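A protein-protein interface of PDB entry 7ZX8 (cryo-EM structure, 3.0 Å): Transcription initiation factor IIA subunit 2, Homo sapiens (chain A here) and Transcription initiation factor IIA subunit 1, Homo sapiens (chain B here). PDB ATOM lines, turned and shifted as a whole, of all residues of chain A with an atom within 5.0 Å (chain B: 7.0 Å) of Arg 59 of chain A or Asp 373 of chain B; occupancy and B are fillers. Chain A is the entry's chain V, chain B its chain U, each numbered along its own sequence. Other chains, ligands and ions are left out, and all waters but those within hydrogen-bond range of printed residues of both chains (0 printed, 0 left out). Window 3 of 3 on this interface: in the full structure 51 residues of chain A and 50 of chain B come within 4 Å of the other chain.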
ATOM      1  N   ASN A  57     -28.339  -5.655   6.791  1.00  0.00           N
ATOM      2  CA  ASN A  57     -27.461  -4.991   7.748  1.00  0.00           C
ATOM      3  C   ASN A  57     -26.786  -3.833   7.034  1.00  0.00           C
ATOM      4  O   ASN A  57     -26.112  -4.042   6.021  1.00  0.00           O
ATOM      5  CB  ASN A  57     -26.417  -5.959   8.309  1.00  0.00           C
ATOM      6  CG  ASN A  57     -27.025  -7.014   9.212  1.00  0.00           C
ATOM      7  OD1 ASN A  57     -27.883  -6.718  10.043  1.00  0.00           O
ATOM      8  ND2 ASN A  57     -26.579  -8.254   9.054  1.00  0.00           N
ATOM      9  N   PHE A  58     -26.967  -2.620   7.569  1.00  0.00           N
ATOM     10  CA  PHE A  58     -26.458  -1.414   6.862  1.00  0.00           C
ATOM     11  C   PHE A  58     -25.367  -0.689   7.655  1.00  0.00           C
ATOM     12  O   PHE A  58     -25.446  -0.656   8.895  1.00  0.00           O
ATOM     13  CB  PHE A  58     -27.623  -0.478   6.520  1.00  0.00           C
ATOM     14  CG  PHE A  58     -28.530  -0.107   7.667  1.00  0.00           C
ATOM     15  CD1 PHE A  58     -29.608  -0.907   8.013  1.00  0.00           C
ATOM     16  CD2 PHE A  58     -28.321   1.058   8.387  1.00  0.00           C
ATOM     17  CE1 PHE A  58     -30.441  -0.561   9.065  1.00  0.00           C
ATOM     18  CE2 PHE A  58     -29.156   1.405   9.436  1.00  0.00           C
ATOM     19  CZ  PHE A  58     -30.215   0.595   9.774  1.00  0.00           C
ATOM     20  N   ARG A  59     -24.371  -0.134   6.955  1.00  0.00           N
ATOM     21  CA  ARG A  59     -23.317   0.676   7.626  1.00  0.00           C
ATOM     22  C   ARG A  59     -23.305   2.066   6.986  1.00  0.00           C
ATOM     23  O   ARG A  59     -23.234   2.133   5.745  1.00  0.00           O
ATOM     24  CB  ARG A  59     -21.942   0.016   7.486  1.00  0.00           C
ATOM     25  CG  ARG A  59     -21.891  -1.435   7.941  1.00  0.00           C
ATOM     26  CD  ARG A  59     -21.472  -2.327   6.791  1.00  0.00           C
ATOM     27  NE  ARG A  59     -21.982  -3.683   6.912  1.00  0.00           N
ATOM     28  CZ  ARG A  59     -22.995  -4.172   6.209  1.00  0.00           C
ATOM     29  NH1 ARG A  59     -23.615  -3.409   5.325  1.00  0.00           N
ATOM     30  NH2 ARG A  59     -23.381  -5.421   6.388  1.00  0.00           N
ATOM     31  N   GLY A  60     -23.348   3.128   7.795  1.00  0.00           N
ATOM     32  CA  GLY A  60     -23.424   4.499   7.251  1.00  0.00           C
ATOM     33  C   GLY A  60     -22.869   5.519   8.227  1.00  0.00           C
ATOM     34  O   GLY A  60     -22.529   5.120   9.347  1.00  0.00           O
ATOM     35  N   SER A  61     -22.703   6.773   7.797  1.00  0.00           N
ATOM     36  CA  SER A  61     -22.265   7.837   8.740  1.00  0.00           C
ATOM     37  C   SER A  61     -23.471   8.714   9.095  1.00  0.00           C
ATOM     38  O   SER A  61     -23.934   9.453   8.203  1.00  0.00           O
ATOM     39  CB  SER A  61     -21.145   8.653   8.151  1.00  0.00           C
ATOM     40  OG  SER A  61     -21.379   8.911   6.774  1.00  0.00           O
ATOM     41  N   ASP A  78     -23.945   8.177   2.600  1.00  0.00           N
ATOM     42  CA  ASP A  78     -23.034   7.198   2.013  1.00  0.00           C
ATOM     43  C   ASP A  78     -23.232   5.818   2.627  1.00  0.00           C
ATOM     44  O   ASP A  78     -22.280   5.116   2.964  1.00  0.00           O
ATOM     45  CB  ASP A  78     -21.588   7.653   2.168  1.00  0.00           C
ATOM     46  CG  ASP A  78     -21.370   9.076   1.702  1.00  0.00           C
ATOM     47  OD1 ASP A  78     -22.093   9.522   0.789  1.00  0.00           O
ATOM     48  OD2 ASP A  78     -20.476   9.754   2.252  1.00  0.00           O
ATOM     49  N   VAL A  79     -24.483   5.430   2.769  1.00  0.00           N
ATOM     50  CA  VAL A  79     -24.798   4.212   3.504  1.00  0.00           C
ATOM     51  C   VAL A  79     -25.009   3.051   2.543  1.00  0.00           C
ATOM     52  O   VAL A  79     -25.574   3.195   1.452  1.00  0.00           O
ATOM     53  CB  VAL A  79     -26.024   4.440   4.405  1.00  0.00           C
ATOM     54  CG1 VAL A  79     -27.146   4.958   3.593  1.00  0.00           C
ATOM     55  CG2 VAL A  79     -26.439   3.158   5.085  1.00  0.00           C
ATOM     56  N   GLU A  80     -24.556   1.879   2.975  1.00  0.00           N
ATOM     57  CA  GLU A  80     -24.661   0.640   2.221  1.00  0.00           C
ATOM     58  C   GLU A  80     -25.613  -0.292   2.952  1.00  0.00           C
ATOM     59  O   GLU A  80     -25.589  -0.374   4.185  1.00  0.00           O
ATOM     60  CB  GLU A  80     -23.290  -0.012   2.055  1.00  0.00           C
ATOM     61  CG  GLU A  80     -22.601  -0.305   3.371  1.00  0.00           C
ATOM     62  CD  GLU A  80     -21.092  -0.250   3.268  1.00  0.00           C
ATOM     63  OE1 GLU A  80     -20.568   0.768   2.776  1.00  0.00           O
ATOM     64  OE2 GLU A  80     -20.431  -1.222   3.689  1.00  0.00           O
ATOM     65  N   PHE A  81     -26.454  -0.975   2.194  1.00  0.00           N
ATOM     66  CA  PHE A  81     -27.445  -1.905   2.710  1.00  0.00           C
ATOM     67  C   PHE A  81     -27.096  -3.282   2.174  1.00  0.00           C
ATOM     68  O   PHE A  81     -27.254  -3.546   0.977  1.00  0.00           O
ATOM     69  CB  PHE A  81     -28.854  -1.508   2.284  1.00  0.00           C
ATOM     70  CG  PHE A  81     -29.368  -0.279   2.962  1.00  0.00           C
ATOM     71  CD1 PHE A  81     -30.428  -0.357   3.839  1.00  0.00           C
ATOM     72  CD2 PHE A  81     -28.800   0.954   2.717  1.00  0.00           C
ATOM     73  CE1 PHE A  81     -30.900   0.767   4.462  1.00  0.00           C
ATOM     74  CE2 PHE A  81     -29.272   2.079   3.336  1.00  0.00           C
ATOM     75  CZ  PHE A  81     -30.324   1.987   4.208  1.00  0.00           C
ATOM     76  N   ARG A  82     -26.596  -4.140   3.046  1.00  0.00           N
ATOM     77  CA  ARG A  82     -26.337  -5.527   2.702  1.00  0.00           C
ATOM     78  C   ARG A  82     -27.632  -6.301   2.882  1.00  0.00           C
ATOM     79  O   ARG A  82     -28.033  -6.607   4.008  1.00  0.00           O
ATOM     80  CB  ARG A  82     -25.222  -6.110   3.561  1.00  0.00           C
ATOM     81  CG  ARG A  82     -23.830  -5.928   2.982  1.00  0.00           C
ATOM     82  CD  ARG A  82     -23.735  -6.475   1.570  1.00  0.00           C
ATOM     83  NE  ARG A  82     -24.467  -7.722   1.403  1.00  0.00           N
ATOM     84  CZ  ARG A  82     -23.938  -8.923   1.584  1.00  0.00           C
ATOM     85  NH1 ARG A  82     -24.675 -10.012   1.413  1.00  0.00           N
ATOM     86  NH2 ARG A  82     -22.666  -9.035   1.933  1.00  0.00           N
ATOM     87  N   ASN B 347     -20.493   7.961  20.034  1.00  0.00           N
ATOM     88  CA  ASN B 347     -20.625   8.288  18.626  1.00  0.00           C
ATOM     89  C   ASN B 347     -21.370   7.214  17.866  1.00  0.00           C
ATOM     90  O   ASN B 347     -22.002   7.506  16.849  1.00  0.00           O
ATOM     91  CB  ASN B 347     -19.249   8.495  17.993  1.00  0.00           C
ATOM     92  CG  ASN B 347     -18.728   9.899  18.181  1.00  0.00           C
ATOM     93  OD1 ASN B 347     -17.882  10.147  19.038  1.00  0.00           O
ATOM     94  ND2 ASN B 347     -19.222  10.829  17.376  1.00  0.00           N
ATOM     95  N   LYS B 348     -21.319   5.982  18.353  1.00  0.00           N
ATOM     96  CA  LYS B 348     -21.696   4.820  17.569  1.00  0.00           C
ATOM     97  C   LYS B 348     -23.157   4.505  17.805  1.00  0.00           C
ATOM     98  O   LYS B 348     -23.536   4.076  18.896  1.00  0.00           O
ATOM     99  CB  LYS B 348     -20.831   3.617  17.930  1.00  0.00           C
ATOM    100  CG  LYS B 348     -19.345   3.858  17.754  1.00  0.00           C
ATOM    101  CD  LYS B 348     -18.981   4.095  16.299  1.00  0.00           C
ATOM    102  CE  LYS B 348     -19.586   3.043  15.373  1.00  0.00           C
ATOM    103  NZ  LYS B 348     -19.348   1.647  15.831  1.00  0.00           N
ATOM    104  N   TRP B 349     -23.971   4.734  16.791  1.00  0.00           N
ATOM    105  CA  TRP B 349     -25.389   4.437  16.846  1.00  0.00           C
ATOM    106  C   TRP B 349     -25.579   3.035  16.311  1.00  0.00           C
ATOM    107  O   TRP B 349     -25.051   2.694  15.250  1.00  0.00           O
ATOM    108  CB  TRP B 349     -26.180   5.446  16.037  1.00  0.00           C
ATOM    109  CG  TRP B 349     -26.232   6.752  16.686  1.00  0.00           C
ATOM    110  CD1 TRP B 349     -25.244   7.681  16.733  1.00  0.00           C
ATOM    111  CD2 TRP B 349     -27.328   7.287  17.415  1.00  0.00           C
ATOM    112  NE1 TRP B 349     -25.664   8.774  17.442  1.00  0.00           N
ATOM    113  CE2 TRP B 349     -26.943   8.554  17.871  1.00  0.00           C
ATOM    114  CE3 TRP B 349     -28.604   6.821  17.722  1.00  0.00           C
ATOM    115  CZ2 TRP B 349     -27.784   9.357  18.612  1.00  0.00           C
ATOM    116  CZ3 TRP B 349     -29.433   7.614  18.455  1.00  0.00           C
ATOM    117  CH2 TRP B 349     -29.025   8.869  18.898  1.00  0.00           C
ATOM    118  N   LYS B 350     -26.309   2.223  17.048  1.00  0.00           N
ATOM    119  CA  LYS B 350     -26.645   0.888  16.598  1.00  0.00           C
ATOM    120  C   LYS B 350     -28.157   0.757  16.581  1.00  0.00           C
ATOM    121  O   LYS B 350     -28.803   0.811  17.632  1.00  0.00           O
ATOM    122  CB  LYS B 350     -26.013  -0.164  17.502  1.00  0.00           C
ATOM    123  CG  LYS B 350     -26.426  -1.575  17.173  1.00  0.00           C
ATOM    124  CD  LYS B 350     -25.334  -2.571  17.530  1.00  0.00           C
ATOM    125  CE  LYS B 350     -24.599  -2.180  18.808  1.00  0.00           C
ATOM    126  NZ  LYS B 350     -25.469  -2.234  20.014  1.00  0.00           N
ATOM    127  N   PHE B 351     -28.715   0.624  15.388  1.00  0.00           N
ATOM    128  CA  PHE B 351     -30.146   0.510  15.194  1.00  0.00           C
ATOM    129  C   PHE B 351     -30.514  -0.953  15.048  1.00  0.00           C
ATOM    130  O   PHE B 351     -29.833  -1.702  14.356  1.00  0.00           O
ATOM    131  CB  PHE B 351     -30.598   1.262  13.947  1.00  0.00           C
ATOM    132  CG  PHE B 351     -29.829   2.503  13.688  1.00  0.00           C
ATOM    133  CD1 PHE B 351     -30.152   3.672  14.321  1.00  0.00           C
ATOM    134  CD2 PHE B 351     -28.774   2.498  12.814  1.00  0.00           C
ATOM    135  CE1 PHE B 351     -29.437   4.811  14.079  1.00  0.00           C
ATOM    136  CE2 PHE B 351     -28.057   3.635  12.573  1.00  0.00           C
ATOM    137  CZ  PHE B 351     -28.388   4.791  13.203  1.00  0.00           C
ATOM    138  N   ILE B 371     -30.548  -4.879  11.415  1.00  0.00           N
ATOM    139  CA  ILE B 371     -29.531  -4.319  12.282  1.00  0.00           C
ATOM    140  C   ILE B 371     -28.709  -3.344  11.462  1.00  0.00           C
ATOM    141  O   ILE B 371     -28.594  -3.478  10.243  1.00  0.00           O
ATOM    142  CB  ILE B 371     -28.672  -5.442  12.882  1.00  0.00           C
ATOM    143  CG1 ILE B 371     -29.572  -6.454  13.592  1.00  0.00           C
ATOM    144  CG2 ILE B 371     -27.660  -4.887  13.853  1.00  0.00           C
ATOM    145  CD1 ILE B 371     -29.804  -7.724  12.814  1.00  0.00           C
ATOM    146  N   GLY B 372     -28.163  -2.337  12.113  1.00  0.00           N
ATOM    147  CA  GLY B 372     -27.377  -1.352  11.400  1.00  0.00           C
ATOM    148  C   GLY B 372     -26.494  -0.574  12.339  1.00  0.00           C
ATOM    149  O   GLY B 372     -26.786  -0.446  13.529  1.00  0.00           O
ATOM    150  N   ASP B 373     -25.415  -0.033  11.793  1.00  0.00           N
ATOM    151  CA  ASP B 373     -24.467   0.758  12.556  1.00  0.00           C
ATOM    152  C   ASP B 373     -24.333   2.113  11.891  1.00  0.00           C
ATOM    153  O   ASP B 373     -24.679   2.267  10.717  1.00  0.00           O
ATOM    154  CB  ASP B 373     -23.110   0.060  12.638  1.00  0.00           C
ATOM    155  CG  ASP B 373     -22.148   0.745  13.596  1.00  0.00           C
ATOM    156  OD1 ASP B 373     -21.503   0.038  14.402  1.00  0.00           O
ATOM    157  OD2 ASP B 373     -22.022   1.985  13.544  1.00  0.00           O
ATOM    158  N   ALA B 374     -23.845   3.096  12.642  1.00  0.00           N
ATOM    159  CA  ALA B 374     -23.567   4.407  12.090  1.00  0.00           C
ATOM    160  C   ALA B 374     -22.641   5.168  13.020  1.00  0.00           C
ATOM    161  O   ALA B 374     -22.649   4.975  14.235  1.00  0.00           O
ATOM    162  CB  ALA B 374     -24.850   5.206  11.861  1.00  0.00           C
ATOM    163  N   GLU B 375     -21.837   6.043  12.431  1.00  0.00           N
ATOM    164  CA  GLU B 375     -20.940   6.915  13.173  1.00  0.00           C
ATOM    165  C   GLU B 375     -21.411   8.348  13.013  1.00  0.00           C
ATOM    166  O   GLU B 375     -21.598   8.819  11.888  1.00  0.00           O
ATOM    167  CB  GLU B 375     -19.499   6.782  12.692  1.00  0.00           C
ATOM    168  CG  GLU B 375     -18.542   7.680  13.456  1.00  0.00           C
ATOM    169  CD  GLU B 375     -17.109   7.574  12.975  1.00  0.00           C
ATOM    170  OE1 GLU B 375     -16.859   6.807  12.023  1.00  0.00           O
ATOM    171  OE2 GLU B 375     -16.237   8.263  13.547  1.00  0.00           O
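The backbone NH (N) of Gly 372 of chain B sits at hydrogen-bond distance from the backbone carbonyl oxygen (O) of Phe 351 of chain B (2.9 Å).
The backbone NH (N) of Arg 59 of chain A is in hydrogen-bond range of the backbone carbonyl oxygen (O) of Glu 80 of chain A, 3.0 Å away.
The backbone carbonyl oxygen (O) of Asn 57 of chain A sits at hydrogen-bond distance from the guanidinium group (NH1) of Arg 59 of chain A (2.7 Å).
O of Arg 82 of chain A is in hydrogen-bond range of N of Asn 57 of chain A, 3.0 Å away.
The side-chain amino group (NZ) of Lys 348 of chain B lies within salt-bridge range of the side-chain carboxylate (OD1) of Asp 373 of chain B (3.0 Å).
N of Trp 349 of chain B lies within hydrogen-bond range of O of Ala 374 of chain B.
Of the printed residues of chain B, Asn 57 of chain A touches Ile 371.
Arg 59 of chain A touches just one residue of chain B: Asp 373.
Of the printed residues of chain B, Ser 61 of chain A touches Glu 375 (3.4 Å).
Asp 78 of chain A touches none of the printed residues of chain B.
Of the printed residues of chain A, Gly 372 of chain B touches Phe 58 (3.2 Å).
Asp 373 of chain B touches just these residues of chain A: Phe 58 (3.0 Å), Arg 59 (3.7 Å) and Gly 60 (3.3 Å).
The nearest residue of chain B that does not touch Arg 59 of chain A is Gly 372 of chain B (5.5 Å).
The nearest printed residue of chain A that does not touch Glu 375 of chain B is Arg 59 of chain A (6.9 Å).
Printed residues of chain B that touch a printed residue of chain A: Phe 351, Ile 371, Gly 372, Asp 373, Ala 374 and Glu 375.
Hydrophobic or aromatic side chains of chain B within 4 Å of the printed part of chain A: Phe 351, Ile 371 and Ala 374.
Among the printed residues, 10 pairs touch across the chains.
Among the printed residues, no Asp or Glu carboxylate lies within 4 Å of a Lys or Arg side-chain nitrogen of the other chain.
The backbone NH (N) of Phe 58 of chain A sits at hydrogen-bond distance from the backbone carbonyl oxygen (O) of Ile 371 of chain B, at 3.2 Å.
OD1 of Asn 57 of chain A sits close to O of Ile 371 of chain B (3.3 Å).
O of Asp 373 of chain B sits at hydrogen-bond distance from N of Gly 60 of chain A (3.3 Å).
O of Phe 58 of chain A sits at hydrogen-bond distance from N of Asp 373 of chain B (3.0 Å).
The backbone NH (N) of Glu 375 of chain B sits at hydrogen-bond distance from the backbone carbonyl oxygen (O) of Gly 60 of chain A (3.3 Å).
Among the printed residues, pairs that only touch across the chains: Gly 60 of chain A with Ala 374 of chain B (3.0 Å), Phe 58 of chain A with Gly 372 of chain B (3.2 Å), Ser 61 of chain A with Glu 375 of chain B (3.4 Å), Phe 58 of chain A with Phe 351 of chain B (3.6 Å) and Arg 59 of chain A with Asp 373 of chain B (3.7 Å).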
